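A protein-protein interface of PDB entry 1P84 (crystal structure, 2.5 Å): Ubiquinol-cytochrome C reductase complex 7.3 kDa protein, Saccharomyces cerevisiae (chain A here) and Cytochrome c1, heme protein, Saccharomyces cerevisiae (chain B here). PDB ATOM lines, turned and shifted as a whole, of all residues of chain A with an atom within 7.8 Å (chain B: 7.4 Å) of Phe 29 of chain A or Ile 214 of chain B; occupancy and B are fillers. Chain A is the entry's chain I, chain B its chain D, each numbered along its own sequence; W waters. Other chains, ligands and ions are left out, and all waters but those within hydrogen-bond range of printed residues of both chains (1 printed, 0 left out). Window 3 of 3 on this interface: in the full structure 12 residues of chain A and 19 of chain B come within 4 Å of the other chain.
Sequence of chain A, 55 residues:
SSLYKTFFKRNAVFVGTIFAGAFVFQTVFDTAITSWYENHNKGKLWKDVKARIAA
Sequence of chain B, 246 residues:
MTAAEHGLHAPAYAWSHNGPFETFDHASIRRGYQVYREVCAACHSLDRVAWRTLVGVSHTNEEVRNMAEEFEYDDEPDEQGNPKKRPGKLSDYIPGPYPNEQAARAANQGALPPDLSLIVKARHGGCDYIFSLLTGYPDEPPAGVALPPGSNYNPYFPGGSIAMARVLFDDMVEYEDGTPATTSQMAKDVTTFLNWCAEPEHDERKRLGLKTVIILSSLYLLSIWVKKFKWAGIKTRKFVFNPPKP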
ATOM      1  N   ALA A  22     -19.848 -16.238 -21.419  1.00  0.00           N
ATOM      2  CA  ALA A  22     -20.481 -16.568 -20.140  1.00  0.00           C
ATOM      3  C   ALA A  22     -20.013 -17.922 -19.613  1.00  0.00           C
ATOM      4  O   ALA A  22     -19.754 -18.067 -18.418  1.00  0.00           O
ATOM      5  CB  ALA A  22     -22.002 -16.551 -20.281  1.00  0.00           C
ATOM      6  N   PHE A  23     -19.899 -18.904 -20.506  1.00  0.00           N
ATOM      7  CA  PHE A  23     -19.445 -20.243 -20.128  1.00  0.00           C
ATOM      8  C   PHE A  23     -17.980 -20.226 -19.671  1.00  0.00           C
ATOM      9  O   PHE A  23     -17.593 -20.960 -18.757  1.00  0.00           O
ATOM     10  CB  PHE A  23     -19.621 -21.231 -21.289  1.00  0.00           C
ATOM     11  CG  PHE A  23     -21.052 -21.655 -21.526  1.00  0.00           C
ATOM     12  CD1 PHE A  23     -21.398 -23.008 -21.528  1.00  0.00           C
ATOM     13  CD2 PHE A  23     -22.050 -20.710 -21.774  1.00  0.00           C
ATOM     14  CE1 PHE A  23     -22.722 -23.416 -21.778  1.00  0.00           C
ATOM     15  CE2 PHE A  23     -23.373 -21.103 -22.025  1.00  0.00           C
ATOM     16  CZ  PHE A  23     -23.708 -22.458 -22.027  1.00  0.00           C
ATOM     17  N   VAL A  24     -17.172 -19.389 -20.316  1.00  0.00           N
ATOM     18  CA  VAL A  24     -15.764 -19.263 -19.971  1.00  0.00           C
ATOM     19  C   VAL A  24     -15.664 -18.590 -18.608  1.00  0.00           C
ATOM     20  O   VAL A  24     -14.969 -19.083 -17.715  1.00  0.00           O
ATOM     21  CB  VAL A  24     -14.993 -18.409 -21.020  1.00  0.00           C
ATOM     22  CG1 VAL A  24     -13.560 -18.145 -20.561  1.00  0.00           C
ATOM     23  CG2 VAL A  24     -14.984 -19.111 -22.364  1.00  0.00           C
ATOM     24  N   PHE A  25     -16.383 -17.478 -18.456  1.00  0.00           N
ATOM     25  CA  PHE A  25     -16.398 -16.708 -17.213  1.00  0.00           C
ATOM     26  C   PHE A  25     -16.753 -17.560 -15.998  1.00  0.00           C
ATOM     27  O   PHE A  25     -16.057 -17.530 -14.982  1.00  0.00           O
ATOM     28  CB  PHE A  25     -17.392 -15.543 -17.323  1.00  0.00           C
ATOM     29  CG  PHE A  25     -17.504 -14.722 -16.070  1.00  0.00           C
ATOM     30  CD1 PHE A  25     -16.709 -13.599 -15.887  1.00  0.00           C
ATOM     31  CD2 PHE A  25     -18.382 -15.097 -15.050  1.00  0.00           C
ATOM     32  CE1 PHE A  25     -16.782 -12.864 -14.704  1.00  0.00           C
ATOM     33  CE2 PHE A  25     -18.461 -14.370 -13.870  1.00  0.00           C
ATOM     34  CZ  PHE A  25     -17.660 -13.254 -13.696  1.00  0.00           C
ATOM     35  N   GLN A  26     -17.835 -18.323 -16.117  1.00  0.00           N
ATOM     36  CA  GLN A  26     -18.310 -19.170 -15.035  1.00  0.00           C
ATOM     37  C   GLN A  26     -17.245 -20.074 -14.426  1.00  0.00           C
ATOM     38  O   GLN A  26     -17.208 -20.253 -13.212  1.00  0.00           O
ATOM     39  CB  GLN A  26     -19.508 -19.995 -15.503  1.00  0.00           C
ATOM     40  CG  GLN A  26     -20.181 -20.799 -14.401  1.00  0.00           C
ATOM     41  CD  GLN A  26     -21.667 -21.003 -14.653  1.00  0.00           C
ATOM     42  OE1 GLN A  26     -22.467 -20.074 -14.493  1.00  0.00           O
ATOM     43  NE2 GLN A  26     -22.047 -22.218 -15.051  1.00  0.00           N
ATOM     44  N   THR A  27     -16.359 -20.609 -15.259  1.00  0.00           N
ATOM     45  CA  THR A  27     -15.309 -21.505 -14.786  1.00  0.00           C
ATOM     46  C   THR A  27     -14.120 -20.762 -14.177  1.00  0.00           C
ATOM     47  O   THR A  27     -13.642 -21.110 -13.092  1.00  0.00           O
ATOM     48  CB  THR A  27     -14.797 -22.411 -15.932  1.00  0.00           C
ATOM     49  OG1 THR A  27     -15.905 -23.077 -16.551  1.00  0.00           O
ATOM     50  CG2 THR A  27     -13.831 -23.463 -15.392  1.00  0.00           C
ATOM     51  N   VAL A  28     -13.635 -19.756 -14.897  1.00  0.00           N
ATOM     52  CA  VAL A  28     -12.494 -18.954 -14.471  1.00  0.00           C
ATOM     53  C   VAL A  28     -12.754 -18.253 -13.138  1.00  0.00           C
ATOM     54  O   VAL A  28     -11.927 -18.293 -12.219  1.00  0.00           O
ATOM     55  CB  VAL A  28     -12.155 -17.885 -15.539  1.00  0.00           C
ATOM     56  CG1 VAL A  28     -10.946 -17.049 -15.113  1.00  0.00           C
ATOM     57  CG2 VAL A  28     -11.898 -18.558 -16.874  1.00  0.00           C
ATOM     58  N   PHE A  29     -13.914 -17.613 -13.052  1.00  0.00           N
ATOM     59  CA  PHE A  29     -14.335 -16.880 -11.864  1.00  0.00           C
ATOM     60  C   PHE A  29     -14.434 -17.789 -10.637  1.00  0.00           C
ATOM     61  O   PHE A  29     -13.938 -17.441  -9.568  1.00  0.00           O
ATOM     62  CB  PHE A  29     -15.683 -16.201 -12.146  1.00  0.00           C
ATOM     63  CG  PHE A  29     -16.183 -15.333 -11.028  1.00  0.00           C
ATOM     64  CD1 PHE A  29     -15.545 -14.135 -10.720  1.00  0.00           C
ATOM     65  CD2 PHE A  29     -17.310 -15.705 -10.297  1.00  0.00           C
ATOM     66  CE1 PHE A  29     -16.023 -13.320  -9.708  1.00  0.00           C
ATOM     67  CE2 PHE A  29     -17.792 -14.896  -9.284  1.00  0.00           C
ATOM     68  CZ  PHE A  29     -17.148 -13.703  -8.990  1.00  0.00           C
ATOM     69  N   ASP A  30     -15.040 -18.962 -10.806  1.00  0.00           N
ATOM     70  CA  ASP A  30     -15.214 -19.904  -9.703  1.00  0.00           C
ATOM     71  C   ASP A  30     -13.894 -20.394  -9.132  1.00  0.00           C
ATOM     72  O   ASP A  30     -13.780 -20.621  -7.925  1.00  0.00           O
ATOM     73  CB  ASP A  30     -16.058 -21.098 -10.144  1.00  0.00           C
ATOM     74  CG  ASP A  30     -16.427 -22.011  -8.996  1.00  0.00           C
ATOM     75  OD1 ASP A  30     -16.584 -21.523  -7.869  1.00  0.00           O
ATOM     76  OD2 ASP A  30     -16.579 -23.226  -9.217  1.00  0.00           O
ATOM     77  N   THR A  31     -12.899 -20.571  -9.998  1.00  0.00           N
ATOM     78  CA  THR A  31     -11.588 -21.027  -9.549  1.00  0.00           C
ATOM     79  C   THR A  31     -10.900 -19.889  -8.806  1.00  0.00           C
ATOM     80  O   THR A  31     -10.360 -20.088  -7.722  1.00  0.00           O
ATOM     81  CB  THR A  31     -10.718 -21.527 -10.732  1.00  0.00           C
ATOM     82  OG1 THR A  31     -11.235 -22.778 -11.201  1.00  0.00           O
ATOM     83  CG2 THR A  31      -9.266 -21.724 -10.300  1.00  0.00           C
ATOM     84  N   ALA A  32     -10.976 -18.685  -9.367  1.00  0.00           N
ATOM     85  CA  ALA A  32     -10.370 -17.512  -8.743  1.00  0.00           C
ATOM     86  C   ALA A  32     -10.906 -17.289  -7.327  1.00  0.00           C
ATOM     87  O   ALA A  32     -10.135 -17.008  -6.412  1.00  0.00           O
ATOM     88  CB  ALA A  32     -10.608 -16.268  -9.599  1.00  0.00           C
ATOM     89  N   ILE A  33     -12.218 -17.461  -7.150  1.00  0.00           N
ATOM     90  CA  ILE A  33     -12.865 -17.270  -5.856  1.00  0.00           C
ATOM     91  C   ILE A  33     -12.543 -18.379  -4.865  1.00  0.00           C
ATOM     92  O   ILE A  33     -12.152 -18.099  -3.728  1.00  0.00           O
ATOM     93  CB  ILE A  33     -14.400 -17.122  -5.998  1.00  0.00           C
ATOM     94  CG1 ILE A  33     -14.735 -15.883  -6.840  1.00  0.00           C
ATOM     95  CG2 ILE A  33     -15.064 -17.027  -4.622  1.00  0.00           C
ATOM     96  CD1 ILE A  33     -14.209 -14.589  -6.277  1.00  0.00           C
ATOM     97  N   THR A  34     -12.709 -19.632  -5.281  1.00  0.00           N
ATOM     98  CA  THR A  34     -12.410 -20.752  -4.396  1.00  0.00           C
ATOM     99  C   THR A  34     -10.957 -20.675  -3.908  1.00  0.00           C
ATOM    100  O   THR A  34     -10.662 -20.988  -2.751  1.00  0.00           O
ATOM    101  CB  THR A  34     -12.641 -22.094  -5.095  1.00  0.00           C
ATOM    102  OG1 THR A  34     -14.015 -22.195  -5.497  1.00  0.00           O
ATOM    103  CG2 THR A  34     -12.284 -23.256  -4.159  1.00  0.00           C
ATOM    104  N   SER A  35     -10.063 -20.231  -4.793  1.00  0.00           N
ATOM    105  CA  SER A  35      -8.645 -20.088  -4.467  1.00  0.00           C
ATOM    106  C   SER A  35      -8.444 -19.053  -3.377  1.00  0.00           C
ATOM    107  O   SER A  35      -7.973 -19.376  -2.288  1.00  0.00           O
ATOM    108  CB  SER A  35      -7.834 -19.672  -5.700  1.00  0.00           C
ATOM    109  OG  SER A  35      -7.621 -20.773  -6.563  1.00  0.00           O
ATOM    110  N   ARG B 207     -18.980 -18.756   0.746  1.00  0.00           N
ATOM    111  CA  ARG B 207     -18.209 -18.773  -0.500  1.00  0.00           C
ATOM    112  C   ARG B 207     -19.151 -18.358  -1.642  1.00  0.00           C
ATOM    113  O   ARG B 207     -18.817 -17.488  -2.460  1.00  0.00           O
ATOM    114  CB  ARG B 207     -17.652 -20.174  -0.769  1.00  0.00           C
ATOM    115  CG  ARG B 207     -16.512 -20.204  -1.777  1.00  0.00           C
ATOM    116  CD  ARG B 207     -16.220 -21.622  -2.236  1.00  0.00           C
ATOM    117  NE  ARG B 207     -16.733 -21.825  -3.583  1.00  0.00           N
ATOM    118  CZ  ARG B 207     -17.711 -22.662  -3.899  1.00  0.00           C
ATOM    119  NH1 ARG B 207     -18.126 -22.770  -5.155  1.00  0.00           N
ATOM    120  NH2 ARG B 207     -18.259 -23.411  -2.963  1.00  0.00           N
ATOM    121  N   LEU B 208     -20.326 -18.991  -1.692  1.00  0.00           N
ATOM    122  CA  LEU B 208     -21.330 -18.660  -2.704  1.00  0.00           C
ATOM    123  C   LEU B 208     -21.742 -17.187  -2.588  1.00  0.00           C
ATOM    124  O   LEU B 208     -21.979 -16.516  -3.592  1.00  0.00           O
ATOM    125  CB  LEU B 208     -22.560 -19.546  -2.544  1.00  0.00           C
ATOM    126  CG  LEU B 208     -22.377 -21.047  -2.764  1.00  0.00           C
ATOM    127  CD1 LEU B 208     -23.741 -21.720  -2.803  1.00  0.00           C
ATOM    128  CD2 LEU B 208     -21.654 -21.288  -4.075  1.00  0.00           C
ATOM    129  N   GLY B 209     -21.772 -16.685  -1.354  1.00  0.00           N
ATOM    130  CA  GLY B 209     -22.140 -15.306  -1.121  1.00  0.00           C
ATOM    131  C   GLY B 209     -21.184 -14.332  -1.769  1.00  0.00           C
ATOM    132  O   GLY B 209     -21.605 -13.331  -2.348  1.00  0.00           O
ATOM    133  N   LEU B 210     -19.890 -14.623  -1.670  1.00  0.00           N
ATOM    134  CA  LEU B 210     -18.856 -13.771  -2.249  1.00  0.00           C
ATOM    135  C   LEU B 210     -18.998 -13.672  -3.774  1.00  0.00           C
ATOM    136  O   LEU B 210     -18.819 -12.600  -4.348  1.00  0.00           O
ATOM    137  CB  LEU B 210     -17.469 -14.300  -1.853  1.00  0.00           C
ATOM    138  CG  LEU B 210     -16.232 -13.530  -2.341  1.00  0.00           C
ATOM    139  CD1 LEU B 210     -16.297 -12.060  -1.922  1.00  0.00           C
ATOM    140  CD2 LEU B 210     -14.978 -14.197  -1.808  1.00  0.00           C
ATOM    141  N   LYS B 211     -19.342 -14.785  -4.417  1.00  0.00           N
ATOM    142  CA  LYS B 211     -19.522 -14.805  -5.868  1.00  0.00           C
ATOM    143  C   LYS B 211     -20.741 -13.970  -6.233  1.00  0.00           C
ATOM    144  O   LYS B 211     -20.669 -13.091  -7.102  1.00  0.00           O
ATOM    145  CB  LYS B 211     -19.756 -16.230  -6.384  1.00  0.00           C
ATOM    146  CG  LYS B 211     -18.646 -17.243  -6.113  1.00  0.00           C
ATOM    147  CD  LYS B 211     -18.972 -18.594  -6.747  1.00  0.00           C
ATOM    148  CE  LYS B 211     -18.891 -18.529  -8.273  1.00  0.00           C
ATOM    149  NZ  LYS B 211     -19.330 -19.789  -8.952  1.00  0.00           N
ATOM    150  N   THR B 212     -21.855 -14.257  -5.550  1.00  0.00           N
ATOM    151  CA  THR B 212     -23.141 -13.590  -5.762  1.00  0.00           C
ATOM    152  C   THR B 212     -23.068 -12.072  -5.613  1.00  0.00           C
ATOM    153  O   THR B 212     -23.590 -11.320  -6.446  1.00  0.00           O
ATOM    154  CB  THR B 212     -24.202 -14.110  -4.776  1.00  0.00           C
ATOM    155  OG1 THR B 212     -24.297 -15.532  -4.870  1.00  0.00           O
ATOM    156  CG2 THR B 212     -25.548 -13.523  -5.100  1.00  0.00           C
ATOM    157  N   VAL B 213     -22.412 -11.622  -4.555  1.00  0.00           N
ATOM    158  CA  VAL B 213     -22.294 -10.195  -4.307  1.00  0.00           C
ATOM    159  C   VAL B 213     -21.406  -9.460  -5.311  1.00  0.00           C
ATOM    160  O   VAL B 213     -21.662  -8.295  -5.620  1.00  0.00           O
ATOM    161  CB  VAL B 213     -21.878  -9.922  -2.840  1.00  0.00           C
ATOM    162  CG1 VAL B 213     -21.463  -8.475  -2.646  1.00  0.00           C
ATOM    163  CG2 VAL B 213     -23.052 -10.240  -1.926  1.00  0.00           C
ATOM    164  N   ILE B 214     -20.391 -10.134  -5.850  1.00  0.00           N
ATOM    165  CA  ILE B 214     -19.514  -9.493  -6.833  1.00  0.00           C
ATOM    166  C   ILE B 214     -20.226  -9.305  -8.176  1.00  0.00           C
ATOM    167  O   ILE B 214     -20.137  -8.240  -8.792  1.00  0.00           O
ATOM    168  CB  ILE B 214     -18.196 -10.266  -7.021  1.00  0.00           C
ATOM    169  CG1 ILE B 214     -17.282 -10.023  -5.816  1.00  0.00           C
ATOM    170  CG2 ILE B 214     -17.481  -9.830  -8.294  1.00  0.00           C
ATOM    171  CD1 ILE B 214     -15.996 -10.837  -5.845  1.00  0.00           C
ATOM    172  N   ILE B 215     -20.949 -10.327  -8.614  1.00  0.00           N
ATOM    173  CA  ILE B 215     -21.680 -10.248  -9.873  1.00  0.00           C
ATOM    174  C   ILE B 215     -22.791  -9.191  -9.803  1.00  0.00           C
ATOM    175  O   ILE B 215     -22.855  -8.285 -10.654  1.00  0.00           O
ATOM    176  CB  ILE B 215     -22.267 -11.622 -10.249  1.00  0.00           C
ATOM    177  CG1 ILE B 215     -21.129 -12.574 -10.622  1.00  0.00           C
ATOM    178  CG2 ILE B 215     -23.279 -11.493 -11.384  1.00  0.00           C
ATOM    179  CD1 ILE B 215     -21.525 -14.028 -10.602  1.00  0.00           C
ATOM    180  N   LEU B 216     -23.620  -9.263  -8.762  1.00  0.00           N
ATOM    181  CA  LEU B 216     -24.706  -8.308  -8.610  1.00  0.00           C
ATOM    182  C   LEU B 216     -24.221  -6.865  -8.471  1.00  0.00           C
ATOM    183  O   LEU B 216     -24.852  -5.948  -9.009  1.00  0.00           O
ATOM    184  CB  LEU B 216     -25.638  -8.716  -7.464  1.00  0.00           C
ATOM    185  CG  LEU B 216     -26.532  -9.912  -7.817  1.00  0.00           C
ATOM    186  CD1 LEU B 216     -27.151 -10.534  -6.577  1.00  0.00           C
ATOM    187  CD2 LEU B 216     -27.593  -9.485  -8.805  1.00  0.00           C
ATOM    188  N   SER B 217     -23.091  -6.666  -7.791  1.00  0.00           N
ATOM    189  CA  SER B 217     -22.539  -5.319  -7.620  1.00  0.00           C
ATOM    190  C   SER B 217     -22.184  -4.777  -8.982  1.00  0.00           C
ATOM    191  O   SER B 217     -22.599  -3.676  -9.350  1.00  0.00           O
ATOM    192  CB  SER B 217     -21.284  -5.325  -6.748  1.00  0.00           C
ATOM    193  OG  SER B 217     -21.622  -5.422  -5.378  1.00  0.00           O
ATOM    194  N   SER B 218     -21.465  -5.593  -9.747  1.00  0.00           N
ATOM    195  CA  SER B 218     -21.031  -5.228 -11.090  1.00  0.00           C
ATOM    196  C   SER B 218     -22.221  -4.929 -11.991  1.00  0.00           C
ATOM    197  O   SER B 218     -22.229  -3.919 -12.702  1.00  0.00           O
ATOM    198  CB  SER B 218     -20.174  -6.350 -11.687  1.00  0.00           C
ATOM    199  OG  SER B 218     -18.997  -6.541 -10.915  1.00  0.00           O
ATOM    200  N   LEU B 219     -23.223  -5.807 -11.948  1.00  0.00           N
ATOM    201  CA  LEU B 219     -24.445  -5.649 -12.743  1.00  0.00           C
ATOM    202  C   LEU B 219     -25.139  -4.338 -12.402  1.00  0.00           C
ATOM    203  O   LEU B 219     -25.584  -3.609 -13.299  1.00  0.00           O
ATOM    204  CB  LEU B 219     -25.401  -6.807 -12.471  1.00  0.00           C
ATOM    205  CG  LEU B 219     -25.643  -7.855 -13.556  1.00  0.00           C
ATOM    206  CD1 LEU B 219     -24.706  -7.660 -14.732  1.00  0.00           C
ATOM    207  CD2 LEU B 219     -25.526  -9.238 -12.958  1.00  0.00           C
ATOM    208  N   TYR B 220     -25.193  -4.026 -11.104  1.00  0.00           N
ATOM    209  CA  TYR B 220     -25.821  -2.804 -10.634  1.00  0.00           C
ATOM    210  C   TYR B 220     -25.125  -1.564 -11.189  1.00  0.00           C
ATOM    211  O   TYR B 220     -25.781  -0.660 -11.719  1.00  0.00           O
ATOM    212  CB  TYR B 220     -25.849  -2.773  -9.109  1.00  0.00           C
ATOM    213  CG  TYR B 220     -26.300  -1.454  -8.534  1.00  0.00           C
ATOM    214  CD1 TYR B 220     -27.531  -0.893  -8.890  1.00  0.00           C
ATOM    215  CD2 TYR B 220     -25.487  -0.755  -7.642  1.00  0.00           C
ATOM    216  CE1 TYR B 220     -27.941   0.335  -8.369  1.00  0.00           C
ATOM    217  CE2 TYR B 220     -25.880   0.472  -7.112  1.00  0.00           C
ATOM    218  CZ  TYR B 220     -27.107   1.010  -7.477  1.00  0.00           C
ATOM    219  OH  TYR B 220     -27.490   2.215  -6.935  1.00  0.00           O
HETATM  220  O   HOH W   1     -16.453 -20.449  -5.540  1.00  0.00           O
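OD1 of Asp 30 of chain A is in salt-bridge range of NH1 of Arg 207 of chain B (3.4 Å). OG1 of Thr 34 of chain A lies within hydrogen-bond range of NE of Arg 207 of chain B (3.3 Å). NZ of Lys 211 of chain B is in salt-bridge range of OD1 of Asp 30 of chain A (3.4 Å).
OG of Ser 218 of chain B is in hydrogen-bond range of O of Ile 214 of chain B (2.9 Å). The backbone carbonyl oxygen of Asp 30 of chain A lies within hydrogen-bond range of the side-chain hydroxyl of Thr 34 of chain A (2.9 Å).
Among the printed residues, merely in contact across the chains: Phe 29 of chain A with Lys 211 of chain B (3.7 Å), Phe 29 of chain A with Ile 214 of chain B (3.9 Å), Ile 33 of chain A with Leu 210 of chain B (3.99 Å) and Ile 33 of chain A with Lys 211 of chain B (3.9 Å).
Phe 23 of chain A touches none of the printed residues of chain B. Phe 29 of chain A touches two residues of chain B. Printed residues of chain B within 4 Å of Thr 34 of chain A: Arg 207 (3.3 Å). Of the printed residues of chain A, Arg 207 of chain B touches Asp 30 and Thr 34. Printed residues of chain A within 4 Å of Lys 211 of chain B: Phe 29 (3.7 Å), Asp 30 (3.4 Å) and Ile 33 (3.9 Å). Ile 214 of chain B touches one residue of chain A. Leu 219 of chain B touches none of the printed residues of chain A. The nearest residue of chain B that does not touch Phe 29 of chain A is Ile 215 of chain B (4.1 Å). The nearest printed residue of chain B that does not touch Asp 30 of chain A is Leu 208 of chain B (6.3 Å).
Printed residues of chain B that touch a printed residue of chain A: Arg 207, Leu 210, Lys 211 and Ile 214. Of the 14 printed residues of chain A, 4 touch a printed residue of chain B. Hydrophobic or aromatic side chains of chain A within 4 Å of the printed part of chain B: Phe 29 and Ile 33.
Water W1 lies within hydrogen-bond range of NE of Arg 207 of chain B (2.4 Å), OD1 of Asp 30 of chain A (2.6 Å) and OG1 of Thr 34 of chain A (3.0 Å).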
